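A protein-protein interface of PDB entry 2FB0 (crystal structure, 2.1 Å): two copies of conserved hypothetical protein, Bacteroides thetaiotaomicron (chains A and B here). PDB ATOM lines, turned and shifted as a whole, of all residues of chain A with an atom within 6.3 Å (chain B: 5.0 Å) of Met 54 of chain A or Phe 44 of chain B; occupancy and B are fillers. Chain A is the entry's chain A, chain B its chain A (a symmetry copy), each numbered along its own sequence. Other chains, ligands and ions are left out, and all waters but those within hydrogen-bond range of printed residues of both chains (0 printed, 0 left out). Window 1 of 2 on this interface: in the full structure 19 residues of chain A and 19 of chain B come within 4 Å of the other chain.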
ATOM      1  N   LEU A   7      14.634   4.845   0.186  1.00  0.00           N
ATOM      2  CA  LEU A   7      15.961   5.315  -0.239  1.00  0.00           C
ATOM      3  C   LEU A   7      17.021   4.892   0.757  1.00  0.00           C
ATOM      4  O   LEU A   7      16.811   4.982   1.969  1.00  0.00           O
ATOM      5  CB  LEU A   7      16.007   6.842  -0.417  1.00  0.00           C
ATOM      6  CG  LEU A   7      14.978   7.545  -1.319  1.00  0.00           C
ATOM      7  CD1 LEU A   7      15.324   9.020  -1.444  1.00  0.00           C
ATOM      8  CD2 LEU A   7      14.957   6.921  -2.690  1.00  0.00           C
ATOM      9  N   ASN A   8      18.138   4.403   0.228  1.00  0.00           N
ATOM     10  CA  ASN A   8      19.368   4.214   0.975  1.00  0.00           C
ATOM     11  C   ASN A   8      20.425   5.130   0.354  1.00  0.00           C
ATOM     12  O   ASN A   8      20.840   4.924  -0.791  1.00  0.00           O
ATOM     13  CB  ASN A   8      19.857   2.764   0.893  1.00  0.00           C
ATOM     14  CG  ASN A   8      18.919   1.753   1.593  1.00  0.00           C
ATOM     15  OD1 ASN A   8      17.998   2.120   2.349  1.00  0.00           O
ATOM     16  ND2 ASN A   8      19.155   0.480   1.332  1.00  0.00           N
ATOM     17  N   VAL A   9      20.857   6.133   1.110  1.00  0.00           N
ATOM     18  CA  VAL A   9      21.793   7.132   0.598  1.00  0.00           C
ATOM     19  C   VAL A   9      23.096   6.985   1.365  1.00  0.00           C
ATOM     20  O   VAL A   9      23.162   7.292   2.554  1.00  0.00           O
ATOM     21  CB  VAL A   9      21.224   8.563   0.726  1.00  0.00           C
ATOM     22  CG1 VAL A   9      22.211   9.593   0.145  1.00  0.00           C
ATOM     23  CG2 VAL A   9      19.857   8.680   0.007  1.00  0.00           C
ATOM     24  N   PHE A  10      24.110   6.455   0.690  1.00  0.00           N
ATOM     25  CA  PHE A  10      25.401   6.179   1.312  1.00  0.00           C
ATOM     26  C   PHE A  10      26.304   7.381   1.141  1.00  0.00           C
ATOM     27  O   PHE A  10      26.339   7.985   0.074  1.00  0.00           O
ATOM     28  CB  PHE A  10      26.025   4.919   0.717  1.00  0.00           C
ATOM     29  CG  PHE A  10      25.138   3.706   0.848  1.00  0.00           C
ATOM     30  CD1 PHE A  10      25.127   2.966   2.023  1.00  0.00           C
ATOM     31  CD2 PHE A  10      24.296   3.332  -0.193  1.00  0.00           C
ATOM     32  CE1 PHE A  10      24.294   1.859   2.158  1.00  0.00           C
ATOM     33  CE2 PHE A  10      23.452   2.216  -0.071  1.00  0.00           C
ATOM     34  CZ  PHE A  10      23.456   1.482   1.118  1.00  0.00           C
ATOM     35  N   VAL A  11      26.991   7.743   2.219  1.00  0.00           N
ATOM     36  CA  VAL A  11      27.842   8.929   2.250  1.00  0.00           C
ATOM     37  C   VAL A  11      29.245   8.527   2.702  1.00  0.00           C
ATOM     38  O   VAL A  11      29.414   7.871   3.748  1.00  0.00           O
ATOM     39  CB  VAL A  11      27.284  10.036   3.185  1.00  0.00           C
ATOM     40  CG1 VAL A  11      28.146  11.310   3.110  1.00  0.00           C
ATOM     41  CG2 VAL A  11      25.817  10.377   2.857  1.00  0.00           C
ATOM     42  N   ASP A  42      16.109   8.845   8.750  1.00  0.00           N
ATOM     43  CA  ASP A  42      17.100   8.892   9.822  1.00  0.00           C
ATOM     44  C   ASP A  42      18.511   8.814   9.260  1.00  0.00           C
ATOM     45  O   ASP A  42      18.723   8.322   8.157  1.00  0.00           O
ATOM     46  CB  ASP A  42      16.864   7.767  10.858  1.00  0.00           C
ATOM     47  CG  ASP A  42      17.506   8.062  12.219  1.00  0.00           C
ATOM     48  OD1 ASP A  42      18.000   9.196  12.439  1.00  0.00           O
ATOM     49  OD2 ASP A  42      17.506   7.157  13.090  1.00  0.00           O
ATOM     50  N   THR A  43      19.461   9.292  10.051  1.00  0.00           N
ATOM     51  CA  THR A  43      20.884   9.234   9.737  1.00  0.00           C
ATOM     52  C   THR A  43      21.524   8.132  10.573  1.00  0.00           C
ATOM     53  O   THR A  43      21.275   8.061  11.770  1.00  0.00           O
ATOM     54  CB  THR A  43      21.522  10.608  10.051  1.00  0.00           C
ATOM     55  OG1 THR A  43      20.817  11.612   9.305  1.00  0.00           O
ATOM     56  CG2 THR A  43      23.011  10.625   9.703  1.00  0.00           C
ATOM     57  N   PHE A  44      22.324   7.275   9.932  1.00  0.00           N
ATOM     58  CA  PHE A  44      22.970   6.135  10.573  1.00  0.00           C
ATOM     59  C   PHE A  44      24.462   6.134  10.248  1.00  0.00           C
ATOM     60  O   PHE A  44      24.838   6.199   9.075  1.00  0.00           O
ATOM     61  CB  PHE A  44      22.411   4.807  10.034  1.00  0.00           C
ATOM     62  CG  PHE A  44      20.959   4.580  10.316  1.00  0.00           C
ATOM     63  CD1 PHE A  44      20.562   3.815  11.421  1.00  0.00           C
ATOM     64  CD2 PHE A  44      19.983   5.094   9.467  1.00  0.00           C
ATOM     65  CE1 PHE A  44      19.205   3.593  11.682  1.00  0.00           C
ATOM     66  CE2 PHE A  44      18.622   4.867   9.727  1.00  0.00           C
ATOM     67  CZ  PHE A  44      18.242   4.110  10.842  1.00  0.00           C
ATOM     68  N   GLU A  45      25.296   5.985  11.266  1.00  0.00           N
ATOM     69  CA  GLU A  45      26.745   5.902  11.088  1.00  0.00           C
ATOM     70  C   GLU A  45      27.199   4.447  11.084  1.00  0.00           C
ATOM     71  O   GLU A  45      26.757   3.652  11.922  1.00  0.00           O
ATOM     72  CB  GLU A  45      27.442   6.615  12.241  1.00  0.00           C
ATOM     73  CG  GLU A  45      27.056   8.066  12.380  1.00  0.00           C
ATOM     74  CD  GLU A  45      27.393   8.637  13.749  1.00  0.00           C
ATOM     75  OE1 GLU A  45      28.503   8.366  14.258  1.00  0.00           O
ATOM     76  OE2 GLU A  45      26.547   9.370  14.298  1.00  0.00           O
ATOM     77  N   SER A  46      28.107   4.105  10.179  1.00  0.00           N
ATOM     78  CA  SER A  46      28.666   2.763  10.165  1.00  0.00           C
ATOM     79  C   SER A  46      29.416   2.484  11.458  1.00  0.00           C
ATOM     80  O   SER A  46      30.190   3.326  11.939  1.00  0.00           O
ATOM     81  CB  SER A  46      29.582   2.543   8.963  1.00  0.00           C
ATOM     82  OG  SER A  46      30.297   1.331   9.085  1.00  0.00           O
ATOM     83  N   SER A  47      29.147   1.296  12.010  1.00  0.00           N
ATOM     84  CA  SER A  47      29.779   0.803  13.235  1.00  0.00           C
ATOM     85  C   SER A  47      31.168   0.235  12.945  1.00  0.00           C
ATOM     86  O   SER A  47      31.940  -0.004  13.877  1.00  0.00           O
ATOM     87  CB  SER A  47      28.912  -0.308  13.869  1.00  0.00           C
ATOM     88  OG  SER A  47      27.676   0.198  14.356  1.00  0.00           O
ATOM     89  N   ARG A  49      33.107   1.232   9.746  1.00  0.00           N
ATOM     90  CA  ARG A  49      33.882   2.113   8.847  1.00  0.00           C
ATOM     91  C   ARG A  49      33.625   3.573   9.213  1.00  0.00           C
ATOM     92  O   ARG A  49      32.548   4.115   8.942  1.00  0.00           O
ATOM     93  CB  ARG A  49      33.496   1.874   7.383  1.00  0.00           C
ATOM     94  CG  ARG A  49      33.750   0.458   6.891  1.00  0.00           C
ATOM     95  CD  ARG A  49      33.143   0.212   5.515  1.00  0.00           C
ATOM     96  NE  ARG A  49      31.680   0.179   5.537  1.00  0.00           N
ATOM     97  CZ  ARG A  49      30.903   0.277   4.458  1.00  0.00           C
ATOM     98  NH1 ARG A  49      31.429   0.449   3.238  1.00  0.00           N
ATOM     99  NH2 ARG A  49      29.586   0.236   4.598  1.00  0.00           N
ATOM    100  N   VAL A  52      32.111   6.110   6.643  1.00  0.00           N
ATOM    101  CA  VAL A  52      30.844   5.800   5.986  1.00  0.00           C
ATOM    102  C   VAL A  52      29.659   6.076   6.910  1.00  0.00           C
ATOM    103  O   VAL A  52      29.648   5.652   8.066  1.00  0.00           O
ATOM    104  CB  VAL A  52      30.779   4.334   5.461  1.00  0.00           C
ATOM    105  CG1 VAL A  52      29.416   4.060   4.796  1.00  0.00           C
ATOM    106  CG2 VAL A  52      31.904   4.040   4.468  1.00  0.00           C
ATOM    107  N   PHE A  53      28.676   6.816   6.410  1.00  0.00           N
ATOM    108  CA  PHE A  53      27.361   6.847   7.057  1.00  0.00           C
ATOM    109  C   PHE A  53      26.288   6.749   5.986  1.00  0.00           C
ATOM    110  O   PHE A  53      26.610   6.742   4.803  1.00  0.00           O
ATOM    111  CB  PHE A  53      27.189   8.033   8.041  1.00  0.00           C
ATOM    112  CG  PHE A  53      26.999   9.391   7.389  1.00  0.00           C
ATOM    113  CD1 PHE A  53      28.102  10.201   7.090  1.00  0.00           C
ATOM    114  CD2 PHE A  53      25.711   9.883   7.131  1.00  0.00           C
ATOM    115  CE1 PHE A  53      27.922  11.475   6.524  1.00  0.00           C
ATOM    116  CE2 PHE A  53      25.516  11.143   6.567  1.00  0.00           C
ATOM    117  CZ  PHE A  53      26.630  11.953   6.263  1.00  0.00           C
ATOM    118  N   MET A  54      25.029   6.602   6.392  1.00  0.00           N
ATOM    119  CA  MET A  54      23.956   6.454   5.430  1.00  0.00           C
ATOM    120  C   MET A  54      22.694   7.132   5.901  1.00  0.00           C
ATOM    121  O   MET A  54      22.495   7.343   7.102  1.00  0.00           O
ATOM    122  CB  MET A  54      23.702   4.979   5.069  1.00  0.00           C
ATOM    123  CG  MET A  54      23.187   4.099   6.208  1.00  0.00           C
ATOM    124  SD  MET A  54      22.489   2.407   5.503  1.00  0.00           S
ATOM    125  CE  MET A  54      21.024   3.280   4.489  1.00  0.00           C
ATOM    126  N   ILE A  55      21.872   7.519   4.938  1.00  0.00           N
ATOM    127  CA  ILE A  55      20.571   8.092   5.213  1.00  0.00           C
ATOM    128  C   ILE A  55      19.557   7.084   4.697  1.00  0.00           C
ATOM    129  O   ILE A  55      19.624   6.655   3.542  1.00  0.00           O
ATOM    130  CB  ILE A  55      20.369   9.470   4.537  1.00  0.00           C
ATOM    131  CG1 ILE A  55      21.485  10.451   4.944  1.00  0.00           C
ATOM    132  CG2 ILE A  55      19.025  10.064   4.952  1.00  0.00           C
ATOM    133  CD1 ILE A  55      21.452  11.798   4.172  1.00  0.00           C
ATOM    134  N   CYS A  56      18.668   6.656   5.586  1.00  0.00           N
ATOM    135  CA  CYS A  56      17.592   5.743   5.239  1.00  0.00           C
ATOM    136  C   CYS A  56      16.283   6.523   5.246  1.00  0.00           C
ATOM    137  O   CYS A  56      15.984   7.225   6.209  1.00  0.00           O
ATOM    138  CB  CYS A  56      17.522   4.597   6.250  1.00  0.00           C
ATOM    139  SG  CYS A  56      16.489   3.233   5.673  1.00  0.00           S
ATOM    140  N   ASP B  42      26.830  -4.269   6.324  1.00  0.00           N
ATOM    141  CA  ASP B  42      27.401  -3.431   7.376  1.00  0.00           C
ATOM    142  C   ASP B  42      26.370  -3.138   8.456  1.00  0.00           C
ATOM    143  O   ASP B  42      25.170  -3.205   8.214  1.00  0.00           O
ATOM    144  CB  ASP B  42      27.976  -2.115   6.801  1.00  0.00           C
ATOM    145  CG  ASP B  42      29.011  -1.461   7.722  1.00  0.00           C
ATOM    146  OD1 ASP B  42      29.423  -2.083   8.733  1.00  0.00           O
ATOM    147  OD2 ASP B  42      29.436  -0.316   7.428  1.00  0.00           O
ATOM    148  N   THR B  43      26.868  -2.797   9.635  1.00  0.00           N
ATOM    149  CA  THR B  43      26.054  -2.395  10.774  1.00  0.00           C
ATOM    150  C   THR B  43      26.141  -0.881  10.928  1.00  0.00           C
ATOM    151  O   THR B  43      27.235  -0.332  10.880  1.00  0.00           O
ATOM    152  CB  THR B  43      26.578  -3.112  12.042  1.00  0.00           C
ATOM    153  OG1 THR B  43      26.556  -4.526  11.800  1.00  0.00           O
ATOM    154  CG2 THR B  43      25.736  -2.762  13.270  1.00  0.00           C
ATOM    155  N   PHE B  44      24.990  -0.223  11.092  1.00  0.00           N
ATOM    156  CA  PHE B  44      24.894   1.228  11.200  1.00  0.00           C
ATOM    157  C   PHE B  44      24.064   1.604  12.425  1.00  0.00           C
ATOM    158  O   PHE B  44      22.942   1.117  12.583  1.00  0.00           O
ATOM    159  CB  PHE B  44      24.164   1.827   9.985  1.00  0.00           C
ATOM    160  CG  PHE B  44      24.861   1.627   8.677  1.00  0.00           C
ATOM    161  CD1 PHE B  44      25.683   2.632   8.148  1.00  0.00           C
ATOM    162  CD2 PHE B  44      24.676   0.456   7.946  1.00  0.00           C
ATOM    163  CE1 PHE B  44      26.328   2.452   6.920  1.00  0.00           C
ATOM    164  CE2 PHE B  44      25.321   0.277   6.711  1.00  0.00           C
ATOM    165  CZ  PHE B  44      26.148   1.287   6.205  1.00  0.00           C
ATOM    166  N   GLU B  45      24.577   2.516  13.239  1.00  0.00           N
ATOM    167  CA  GLU B  45      23.859   3.012  14.412  1.00  0.00           C
ATOM    168  C   GLU B  45      23.169   4.333  14.094  1.00  0.00           C
ATOM    169  O   GLU B  45      23.767   5.217  13.469  1.00  0.00           O
ATOM    170  CB  GLU B  45      24.846   3.253  15.549  1.00  0.00           C
ATOM    171  CG  GLU B  45      25.626   2.024  15.946  1.00  0.00           C
ATOM    172  CD  GLU B  45      26.880   2.353  16.740  1.00  0.00           C
ATOM    173  OE1 GLU B  45      26.811   3.214  17.647  1.00  0.00           O
ATOM    174  OE2 GLU B  45      27.925   1.733  16.462  1.00  0.00           O
ATOM    175  N   SER B  46      21.935   4.491  14.556  1.00  0.00           N
ATOM    176  CA  SER B  46      21.238   5.754  14.381  1.00  0.00           C
ATOM    177  C   SER B  46      21.970   6.873  15.105  1.00  0.00           C
ATOM    178  O   SER B  46      22.398   6.711  16.259  1.00  0.00           O
ATOM    179  CB  SER B  46      19.789   5.673  14.860  1.00  0.00           C
ATOM    180  OG  SER B  46      19.198   6.956  14.905  1.00  0.00           O
ATOM    181  N   VAL B  52      18.139   2.604  18.375  1.00  0.00           N
ATOM    182  CA  VAL B  52      17.932   2.079  17.027  1.00  0.00           C
ATOM    183  C   VAL B  52      19.261   1.885  16.298  1.00  0.00           C
ATOM    184  O   VAL B  52      20.106   2.781  16.276  1.00  0.00           O
ATOM    185  CB  VAL B  52      16.982   2.972  16.172  1.00  0.00           C
ATOM    186  CG1 VAL B  52      16.817   2.380  14.758  1.00  0.00           C
ATOM    187  CG2 VAL B  52      15.610   3.125  16.829  1.00  0.00           C
ATOM    188  N   PHE B  53      19.459   0.701  15.731  1.00  0.00           N
ATOM    189  CA  PHE B  53      20.511   0.521  14.726  1.00  0.00           C
ATOM    190  C   PHE B  53      19.952  -0.305  13.579  1.00  0.00           C
ATOM    191  O   PHE B  53      18.816  -0.758  13.654  1.00  0.00           O
ATOM    192  CB  PHE B  53      21.841  -0.009  15.318  1.00  0.00           C
ATOM    193  CG  PHE B  53      21.838  -1.477  15.706  1.00  0.00           C
ATOM    194  CD1 PHE B  53      21.463  -1.875  16.995  1.00  0.00           C
ATOM    195  CD2 PHE B  53      22.267  -2.455  14.796  1.00  0.00           C
ATOM    196  CE1 PHE B  53      21.499  -3.230  17.365  1.00  0.00           C
ATOM    197  CE2 PHE B  53      22.304  -3.804  15.147  1.00  0.00           C
ATOM    198  CZ  PHE B  53      21.923  -4.200  16.445  1.00  0.00           C
ATOM    199  N   MET B  54      20.713  -0.439  12.495  1.00  0.00           N
ATOM    200  CA  MET B  54      20.231  -1.172  11.341  1.00  0.00           C
ATOM    201  C   MET B  54      21.343  -1.934  10.666  1.00  0.00           C
ATOM    202  O   MET B  54      22.522  -1.591  10.799  1.00  0.00           O
ATOM    203  CB  MET B  54      19.489  -0.260  10.347  1.00  0.00           C
ATOM    204  CG  MET B  54      20.342   0.811   9.668  1.00  0.00           C
ATOM    205  SD  MET B  54      19.390   1.569   8.130  1.00  0.00           S
ATOM    206  CE  MET B  54      19.372  -0.142   7.127  1.00  0.00           C
ATOM    207  N   CYS B  56      22.389  -3.145   6.927  1.00  0.00           N
ATOM    208  CA  CYS B  56      22.162  -2.969   5.503  1.00  0.00           C
ATOM    209  C   CYS B  56      22.930  -4.055   4.760  1.00  0.00           C
ATOM    210  O   CYS B  56      24.118  -4.255   5.005  1.00  0.00           O
ATOM    211  CB  CYS B  56      22.647  -1.588   5.056  1.00  0.00           C
ATOM    212  SG  CYS B  56      22.046  -1.148   3.411  1.00  0.00           S
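Among the printed residues, merely in contact across the chains: Phe 44 of chain A with Glu 45 of chain B (3.1 Å), Glu 45 of chain A with Phe 44 of chain B (3.1 Å), Phe 44 of chain A with Phe 44 of chain B (3.5 Å), Ser 46 of chain A with Thr 43 of chain B (3.5 Å), Thr 43 of chain A with Ser 46 of chain B (3.5 Å), Phe 44 of chain A with Met 54 of chain B (3.5 Å), Met 54 of chain A with Phe 44 of chain B (3.5 Å), Phe 44 of chain A with Ser 46 of chain B (3.5 Å), Ser 46 of chain A with Phe 44 of chain B (3.5 Å), Phe 10 of chain A with Cys 56 of chain B (3.8 Å), Asn 8 of chain A with Cys 56 of chain B (3.9 Å) and Arg 49 of chain A with Phe 44 of chain B (3.9 Å).
The backbone NH (N) of Asp 42 of chain A lies within hydrogen-bond range of the backbone carbonyl oxygen (O) of Cys 56 of chain A (3.0 Å).
The side-chain hydroxyl of Ser 46 of chain A sits at hydrogen-bond distance from the backbone NH of Arg 49 of chain A (2.9 Å).
The backbone NH (N) of Ser 46 of chain A sits at hydrogen-bond distance from the backbone carbonyl oxygen (O) of Val 52 of chain A, at 3.0 Å.
The backbone carbonyl oxygen (O) of Cys 56 of chain B is in hydrogen-bond range of the backbone NH (N) of Asp 42 of chain B (3.0 Å).
O of Phe 44 of chain B lies within hydrogen-bond range of N of Met 54 of chain B, 2.7 Å away.
N of Ser 46 of chain B sits at hydrogen-bond distance from O of Val 52 of chain B (3.0 Å).
Met 54 of chain A touches just one residue of chain B: Phe 44 (3.5 Å).
Phe 44 of chain B touches five residues of chain A.
Of the printed residues of chain B, Thr 43 of chain A touches Ser 46 (3.5 Å).
Printed residues of chain B within 4 Å of Asp 42 of chain A: Ser 46.
Printed residues of chain A within 4 Å of Cys 56 of chain B: Asn 8 (3.9 Å) and Phe 10 (3.8 Å).
Ile 55 of chain A touches none of the printed residues of chain B.
The nearest residue of chain B that does not touch Met 54 of chain A is Cys 56 of chain B (4.02 Å).
The nearest residue of chain A that does not touch Phe 44 of chain B is Val 52 of chain A (4.1 Å).
The nearest printed residue of chain A that does not touch Glu 45 of chain B is Thr 43 of chain A (4.1 Å).
OD2 of Asp 42 of chain A is in hydrogen-bond range of OG of Ser 46 of chain B.
The backbone carbonyl oxygen (O) of Glu 45 of chain A lies within hydrogen-bond range of the backbone NH (N) of Glu 45 of chain B (2.8 Å).
The side-chain hydroxyl of Ser 46 of chain A is in hydrogen-bond range of the side-chain carboxylate of Asp 42 of chain B, at 2.5 Å.
The backbone NH (N) of Ser 47 of chain A lies within hydrogen-bond range of the backbone carbonyl oxygen (O) of Thr 43 of chain B (2.8 Å).
The side-chain hydroxyl (OG) of Ser 47 of chain A lies within hydrogen-bond range of the side-chain carboxylate (OE2) of Glu 45 of chain B.
The guanidinium group (NH2) of Arg 49 of chain A lies within salt-bridge range of the side-chain carboxylate (OD2) of Asp 42 of chain B, at 2.9 Å.
Of the 17 printed residues of chain A, 10 touch a printed residue of chain B.
Printed residues of chain A that touch a printed residue of chain B: Asn 8, Phe 10, Asp 42, Thr 43, Phe 44, Glu 45, Ser 46, Ser 47, Arg 49 and Met 54.
Hydrophobic or aromatic side chains of chain A within 4 Å of the printed part of chain B: Phe 10, Phe 44 and Met 54.
Of the 9 printed residues of chain B, 7 touch a printed residue of chain A.
Hydrophobic or aromatic side chains of chain B within 4 Å of the printed part of chain A: Phe 44 and Met 54.
Among the printed residues, 18 pairs touch across the chains.
Asp 42 of chain A touches Ser 46 of chain B, and with the chains exchanged Ser 46 of chain A touches Asp 42 of chain B.
Phe 44 of chain A touches its own counterpart, Phe 44 of chain B.
Phe 44 of chain A touches Glu 45 of chain B, and with the chains exchanged Glu 45 of chain A touches Phe 44 of chain B.
Phe 44 of chain A touches Ser 46 of chain B, and with the chains exchanged Ser 46 of chain A touches Phe 44 of chain B.
Positions printed for both chains: 42, 43, 44, 45, 46, 52, 53, 54 and 56.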
